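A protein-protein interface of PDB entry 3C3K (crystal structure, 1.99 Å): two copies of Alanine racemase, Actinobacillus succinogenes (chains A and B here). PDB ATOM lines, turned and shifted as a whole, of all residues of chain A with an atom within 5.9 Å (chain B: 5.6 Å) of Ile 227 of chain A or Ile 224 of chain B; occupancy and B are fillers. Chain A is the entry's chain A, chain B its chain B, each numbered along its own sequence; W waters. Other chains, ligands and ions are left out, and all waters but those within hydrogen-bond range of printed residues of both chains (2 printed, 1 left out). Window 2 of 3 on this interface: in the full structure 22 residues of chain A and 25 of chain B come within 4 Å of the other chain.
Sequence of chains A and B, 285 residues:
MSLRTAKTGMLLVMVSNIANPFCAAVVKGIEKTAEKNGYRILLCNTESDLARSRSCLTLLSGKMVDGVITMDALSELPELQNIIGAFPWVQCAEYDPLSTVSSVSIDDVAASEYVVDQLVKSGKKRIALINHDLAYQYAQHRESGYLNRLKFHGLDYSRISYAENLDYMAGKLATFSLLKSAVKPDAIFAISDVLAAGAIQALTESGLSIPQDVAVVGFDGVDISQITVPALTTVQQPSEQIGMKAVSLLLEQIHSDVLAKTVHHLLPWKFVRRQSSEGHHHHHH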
ATOM      1  N   ASP A 223     -19.827  -9.385   4.610  1.00  0.00           N
ATOM      2  CA  ASP A 223     -19.347 -10.246   5.725  1.00  0.00           C
ATOM      3  C   ASP A 223     -20.418 -10.759   6.642  1.00  0.00           C
ATOM      4  O   ASP A 223     -20.294 -11.863   7.165  1.00  0.00           O
ATOM      5  CB  ASP A 223     -18.314  -9.496   6.586  1.00  0.00           C
ATOM      6  CG  ASP A 223     -17.074  -9.100   5.829  1.00  0.00           C
ATOM      7  OD1 ASP A 223     -16.883  -9.510   4.674  1.00  0.00           O
ATOM      8  OD2 ASP A 223     -16.249  -8.374   6.406  1.00  0.00           O
ATOM      9  N   ILE A 224     -21.505 -10.026   6.839  1.00  0.00           N
ATOM     10  CA  ILE A 224     -22.574 -10.591   7.670  1.00  0.00           C
ATOM     11  C   ILE A 224     -23.118 -11.956   7.211  1.00  0.00           C
ATOM     12  O   ILE A 224     -23.532 -12.771   8.016  1.00  0.00           O
ATOM     13  CB  ILE A 224     -23.758  -9.605   7.907  1.00  0.00           C
ATOM     14  CG1 ILE A 224     -24.474 -10.107   9.162  1.00  0.00           C
ATOM     15  CG2 ILE A 224     -24.665  -9.612   6.705  1.00  0.00           C
ATOM     16  CD1 ILE A 224     -25.441  -9.167   9.805  1.00  0.00           C
ATOM     17  N   SER A 225     -23.101 -12.201   5.916  1.00  0.00           N
ATOM     18  CA  SER A 225     -23.544 -13.452   5.351  1.00  0.00           C
ATOM     19  C   SER A 225     -22.643 -14.614   5.834  1.00  0.00           C
ATOM     20  O   SER A 225     -23.050 -15.752   5.861  1.00  0.00           O
ATOM     21  CB  SER A 225     -23.551 -13.319   3.827  1.00  0.00           C
ATOM     22  OG  SER A 225     -22.230 -13.461   3.282  1.00  0.00           O
ATOM     23  N   GLN A 226     -21.453 -14.306   6.301  1.00  0.00           N
ATOM     24  CA  GLN A 226     -20.560 -15.357   6.858  1.00  0.00           C
ATOM     25  C   GLN A 226     -20.646 -15.513   8.365  1.00  0.00           C
ATOM     26  O   GLN A 226     -20.055 -16.410   8.909  1.00  0.00           O
ATOM     27  CB  GLN A 226     -19.129 -15.126   6.407  1.00  0.00           C
ATOM     28  CG  GLN A 226     -19.075 -15.050   4.894  1.00  0.00           C
ATOM     29  CD  GLN A 226     -17.750 -15.423   4.316  1.00  0.00           C
ATOM     30  OE1 GLN A 226     -17.014 -14.555   3.889  1.00  0.00           O
ATOM     31  NE2 GLN A 226     -17.452 -16.712   4.253  1.00  0.00           N
ATOM     32  N   ILE A 227     -21.442 -14.676   9.022  1.00  0.00           N
ATOM     33  CA  ILE A 227     -21.403 -14.566  10.500  1.00  0.00           C
ATOM     34  C   ILE A 227     -22.651 -15.255  11.111  1.00  0.00           C
ATOM     35  O   ILE A 227     -22.646 -15.761  12.236  1.00  0.00           O
ATOM     36  CB  ILE A 227     -21.289 -13.029  10.934  1.00  0.00           C
ATOM     37  CG1 ILE A 227     -19.867 -12.535  10.867  1.00  0.00           C
ATOM     38  CG2 ILE A 227     -21.789 -12.782  12.358  1.00  0.00           C
ATOM     39  CD1 ILE A 227     -19.722 -11.008  10.562  1.00  0.00           C
ATOM     40  N   THR A 228     -23.724 -15.224  10.323  1.00  0.00           N
ATOM     41  CA  THR A 228     -25.033 -15.749  10.624  1.00  0.00           C
ATOM     42  C   THR A 228     -24.921 -17.303  10.836  1.00  0.00           C
ATOM     43  O   THR A 228     -24.003 -17.931  10.280  1.00  0.00           O
ATOM     44  CB  THR A 228     -25.812 -15.314   9.391  1.00  0.00           C
ATOM     45  OG1 THR A 228     -26.885 -14.394   9.691  1.00  0.00           O
ATOM     46  CG2 THR A 228     -26.051 -16.326   8.399  1.00  0.00           C
ATOM     47  N   VAL A 229     -25.800 -17.885  11.668  1.00  0.00           N
ATOM     48  CA  VAL A 229     -25.917 -19.360  11.855  1.00  0.00           C
ATOM     49  C   VAL A 229     -27.316 -19.845  11.454  1.00  0.00           C
ATOM     50  O   VAL A 229     -28.291 -19.507  12.073  1.00  0.00           O
ATOM     51  CB  VAL A 229     -25.582 -19.820  13.326  1.00  0.00           C
ATOM     52  CG1 VAL A 229     -25.420 -21.350  13.378  1.00  0.00           C
ATOM     53  CG2 VAL A 229     -24.295 -19.189  13.845  1.00  0.00           C
ATOM     54  N   ALA A 231     -24.756 -20.186   7.979  1.00  0.00           N
ATOM     55  CA  ALA A 231     -24.150 -19.217   7.084  1.00  0.00           C
ATOM     56  C   ALA A 231     -25.057 -19.033   5.915  1.00  0.00           C
ATOM     57  O   ALA A 231     -25.810 -19.938   5.537  1.00  0.00           O
ATOM     58  CB  ALA A 231     -22.794 -19.700   6.665  1.00  0.00           C
ATOM     59  N   TYR B 168     -14.415  -8.940  10.576  1.00  0.00           N
ATOM     60  CA  TYR B 168     -14.604 -10.152  11.368  1.00  0.00           C
ATOM     61  C   TYR B 168     -13.427 -11.124  11.115  1.00  0.00           C
ATOM     62  O   TYR B 168     -12.977 -11.759  12.025  1.00  0.00           O
ATOM     63  CB  TYR B 168     -15.975 -10.788  11.088  1.00  0.00           C
ATOM     64  CG  TYR B 168     -15.932 -11.782   9.968  1.00  0.00           C
ATOM     65  CD1 TYR B 168     -15.717 -13.153  10.217  1.00  0.00           C
ATOM     66  CD2 TYR B 168     -16.067 -11.366   8.654  1.00  0.00           C
ATOM     67  CE1 TYR B 168     -15.636 -14.065   9.185  1.00  0.00           C
ATOM     68  CE2 TYR B 168     -16.014 -12.282   7.602  1.00  0.00           C
ATOM     69  CZ  TYR B 168     -15.803 -13.615   7.873  1.00  0.00           C
ATOM     70  OH  TYR B 168     -15.765 -14.490   6.820  1.00  0.00           O
ATOM     71  N   ASP B 193     -17.015  -4.558  18.656  1.00  0.00           N
ATOM     72  CA  ASP B 193     -17.909  -5.669  18.398  1.00  0.00           C
ATOM     73  C   ASP B 193     -17.600  -6.397  17.076  1.00  0.00           C
ATOM     74  O   ASP B 193     -17.859  -7.541  16.975  1.00  0.00           O
ATOM     75  CB  ASP B 193     -19.364  -5.171  18.335  1.00  0.00           C
ATOM     76  CG  ASP B 193     -19.844  -4.629  19.652  1.00  0.00           C
ATOM     77  OD1 ASP B 193     -19.279  -5.023  20.696  1.00  0.00           O
ATOM     78  OD2 ASP B 193     -20.837  -3.895  19.670  1.00  0.00           O
ATOM     79  N   VAL B 194     -17.079  -5.716  16.068  1.00  0.00           N
ATOM     80  CA  VAL B 194     -16.774  -6.351  14.754  1.00  0.00           C
ATOM     81  C   VAL B 194     -15.679  -7.444  14.962  1.00  0.00           C
ATOM     82  O   VAL B 194     -15.762  -8.555  14.442  1.00  0.00           O
ATOM     83  CB  VAL B 194     -16.306  -5.302  13.741  1.00  0.00           C
ATOM     84  CG1 VAL B 194     -15.889  -5.946  12.427  1.00  0.00           C
ATOM     85  CG2 VAL B 194     -17.418  -4.280  13.452  1.00  0.00           C
ATOM     86  N   ALA B 197     -17.084 -10.454  17.014  1.00  0.00           N
ATOM     87  CA  ALA B 197     -17.917 -11.374  16.232  1.00  0.00           C
ATOM     88  C   ALA B 197     -17.029 -12.422  15.558  1.00  0.00           C
ATOM     89  O   ALA B 197     -17.419 -13.581  15.432  1.00  0.00           O
ATOM     90  CB  ALA B 197     -18.732 -10.614  15.209  1.00  0.00           C
ATOM     91  N   GLN B 201     -16.781 -16.524  16.115  1.00  0.00           N
ATOM     92  CA  GLN B 201     -16.617 -17.484  15.023  1.00  0.00           C
ATOM     93  C   GLN B 201     -15.404 -18.419  15.135  1.00  0.00           C
ATOM     94  O   GLN B 201     -15.528 -19.638  14.974  1.00  0.00           O
ATOM     95  CB  GLN B 201     -16.561 -16.779  13.688  1.00  0.00           C
ATOM     96  CG  GLN B 201     -16.609 -17.824  12.585  1.00  0.00           C
ATOM     97  CD  GLN B 201     -16.941 -17.299  11.230  1.00  0.00           C
ATOM     98  OE1 GLN B 201     -16.138 -17.415  10.295  1.00  0.00           O
ATOM     99  NE2 GLN B 201     -18.169 -16.813  11.075  1.00  0.00           N
ATOM    100  N   VAL B 222     -22.842  -1.973  18.732  1.00  0.00           N
ATOM    101  CA  VAL B 222     -23.416  -1.855  17.371  1.00  0.00           C
ATOM    102  C   VAL B 222     -24.286  -3.092  17.067  1.00  0.00           C
ATOM    103  O   VAL B 222     -24.320  -4.013  17.882  1.00  0.00           O
ATOM    104  CB  VAL B 222     -22.350  -1.555  16.299  1.00  0.00           C
ATOM    105  CG1 VAL B 222     -21.801  -0.145  16.488  1.00  0.00           C
ATOM    106  CG2 VAL B 222     -21.145  -2.617  16.358  1.00  0.00           C
ATOM    107  N   ASP B 223     -25.087  -3.060  16.002  1.00  0.00           N
ATOM    108  CA  ASP B 223     -26.052  -4.162  15.741  1.00  0.00           C
ATOM    109  C   ASP B 223     -25.430  -5.556  15.660  1.00  0.00           C
ATOM    110  O   ASP B 223     -26.059  -6.519  16.088  1.00  0.00           O
ATOM    111  CB  ASP B 223     -26.825  -3.973  14.441  1.00  0.00           C
ATOM    112  CG  ASP B 223     -27.851  -2.898  14.545  1.00  0.00           C
ATOM    113  OD1 ASP B 223     -27.915  -2.223  15.610  1.00  0.00           O
ATOM    114  OD2 ASP B 223     -28.563  -2.706  13.546  1.00  0.00           O
ATOM    115  N   ILE B 224     -24.199  -5.679  15.166  1.00  0.00           N
ATOM    116  CA  ILE B 224     -23.594  -7.024  15.071  1.00  0.00           C
ATOM    117  C   ILE B 224     -23.585  -7.712  16.422  1.00  0.00           C
ATOM    118  O   ILE B 224     -23.696  -8.930  16.522  1.00  0.00           O
ATOM    119  CB  ILE B 224     -22.168  -7.060  14.390  1.00  0.00           C
ATOM    120  CG1 ILE B 224     -21.802  -8.486  13.914  1.00  0.00           C
ATOM    121  CG2 ILE B 224     -21.057  -6.627  15.344  1.00  0.00           C
ATOM    122  CD1 ILE B 224     -22.781  -9.070  12.872  1.00  0.00           C
ATOM    123  N   SER B 225     -23.473  -6.924  17.480  1.00  0.00           N
ATOM    124  CA  SER B 225     -23.436  -7.505  18.810  1.00  0.00           C
ATOM    125  C   SER B 225     -24.782  -8.167  19.187  1.00  0.00           C
ATOM    126  O   SER B 225     -24.846  -8.969  20.144  1.00  0.00           O
ATOM    127  CB  SER B 225     -23.000  -6.458  19.820  1.00  0.00           C
ATOM    128  OG  SER B 225     -24.071  -5.585  20.147  1.00  0.00           O
ATOM    129  N   GLN B 226     -25.847  -7.870  18.442  1.00  0.00           N
ATOM    130  CA  GLN B 226     -27.134  -8.510  18.696  1.00  0.00           C
ATOM    131  C   GLN B 226     -27.481  -9.634  17.684  1.00  0.00           C
ATOM    132  O   GLN B 226     -28.574 -10.228  17.719  1.00  0.00           O
ATOM    133  CB  GLN B 226     -28.219  -7.470  18.672  1.00  0.00           C
ATOM    134  CG  GLN B 226     -27.983  -6.420  19.736  1.00  0.00           C
ATOM    135  CD  GLN B 226     -28.922  -5.290  19.557  1.00  0.00           C
ATOM    136  OE1 GLN B 226     -29.132  -4.805  18.438  1.00  0.00           O
ATOM    137  NE2 GLN B 226     -29.517  -4.859  20.635  1.00  0.00           N
ATOM    138  N   ILE B 227     -26.527  -9.893  16.802  1.00  0.00           N
ATOM    139  CA  ILE B 227     -26.672 -10.854  15.765  1.00  0.00           C
ATOM    140  C   ILE B 227     -25.872 -12.140  16.007  1.00  0.00           C
ATOM    141  O   ILE B 227     -26.200 -13.195  15.435  1.00  0.00           O
ATOM    142  CB  ILE B 227     -26.329 -10.237  14.405  1.00  0.00           C
ATOM    143  CG1 ILE B 227     -27.414  -9.257  14.021  1.00  0.00           C
ATOM    144  CG2 ILE B 227     -26.426 -11.300  13.318  1.00  0.00           C
ATOM    145  CD1 ILE B 227     -26.961  -8.186  13.069  1.00  0.00           C
ATOM    146  N   THR B 228     -24.815 -12.047  16.824  1.00  0.00           N
ATOM    147  CA  THR B 228     -23.895 -13.165  16.953  1.00  0.00           C
ATOM    148  C   THR B 228     -24.562 -14.191  17.837  1.00  0.00           C
ATOM    149  O   THR B 228     -25.515 -13.871  18.604  1.00  0.00           O
ATOM    150  CB  THR B 228     -22.558 -12.715  17.571  1.00  0.00           C
ATOM    151  OG1 THR B 228     -22.817 -11.973  18.778  1.00  0.00           O
ATOM    152  CG2 THR B 228     -21.843 -11.840  16.599  1.00  0.00           C
ATOM    153  N   LEU B 232     -23.592 -10.843  22.138  1.00  0.00           N
ATOM    154  CA  LEU B 232     -22.302 -10.344  22.551  1.00  0.00           C
ATOM    155  C   LEU B 232     -22.376  -9.321  23.669  1.00  0.00           C
ATOM    156  O   LEU B 232     -22.984  -8.276  23.490  1.00  0.00           O
ATOM    157  CB  LEU B 232     -21.559  -9.772  21.293  1.00  0.00           C
ATOM    158  CG  LEU B 232     -20.255  -9.143  21.682  1.00  0.00           C
ATOM    159  CD1 LEU B 232     -19.309 -10.301  22.117  1.00  0.00           C
ATOM    160  CD2 LEU B 232     -19.758  -8.320  20.467  1.00  0.00           C
HETATM  161  O   HOH W   1     -20.426 -16.828  13.315  1.00  0.00           O
HETATM  162  O   HOH W   2     -16.482  -7.650   8.871  1.00  0.00           O
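Printed residues of chain A that touch a printed residue of chain B: Asp 223, Ile 224, Gln 226 and Ile 227.
Along chain A the printed residues that touch a printed residue of chain B span positions 223 to 227.
Ile 224 of chain A touches Ile 227 of chain B, and with the chains exchanged Ile 227 of chain A touches Ile 224 of chain B.
Positions printed for both chains: 223, 224, 225, 226, 227 and 228.
Of the 7 pairs that touch across the chains among the printed residues, 2 have their exchanged pair printed and touching as well.
Ile 227 of chain A touches just these residues of chain B: Tyr 168, Gln 201 and Ile 224.
Ile 224 of chain B touches just one residue of chain A: Ile 227.
Of the printed residues of chain B, Asp 223 of chain A touches Tyr 168 (3.6 Å).
Printed residues of chain A within 4 Å of Tyr 168 of chain B: Asp 223, Gln 226 and Ile 227.
Of the printed residues of chain B, Gln 226 of chain A touches Tyr 168 (3.2 Å) and Gln 201 (2.9 Å).
Printed residues of chain A within 4 Å of Ile 227 of chain B: Ile 224.
Of the printed residues of chain B, Ile 224 of chain A touches Ile 227 (3.7 Å).
Ser 225 of chain B touches none of the printed residues of chain A.
The nearest residue of chain B that does not touch Ile 227 of chain A is Thr 228 of chain B (4.3 Å).
The nearest residue of chain A that does not touch Ile 224 of chain B is Ile 224 of chain A (4.1 Å).
The nearest printed residue of chain A that does not touch Gln 201 of chain B is Thr 228 of chain A (5.8 Å).
Asp 223 of chain A touches Tyr 168 of chain B.
Ile 227 of chain B touches Ile 224 of chain A (CD1 to CD1, 3.7 Å).
Ile 227 of chain A touches Tyr 168 of chain B.
CA of Ile 227 of chain A touches NE2 of Gln 201 of chain B, at 3.98 Å.
Ile 227 of chain A touches Ile 224 of chain B.
Water W2 bridges the side-chain carboxylate of Asp 223 of chain A (2.6 Å) and the backbone NH of Tyr 168 of chain B (3.0 Å).
Water W1 lies within hydrogen-bond range of O of Ile 227 of chain A (2.7 Å) and NE2 of Gln 201 of chain B (3.2 Å).
O of Gln 226 of chain A lies within hydrogen-bond range of NE2 of Gln 201 of chain B (2.9 Å).
The side-chain hydroxyl (OH) of Tyr 168 of chain B sits at hydrogen-bond distance from the side-chain amide oxygen (OE1) of Gln 226 of chain A.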
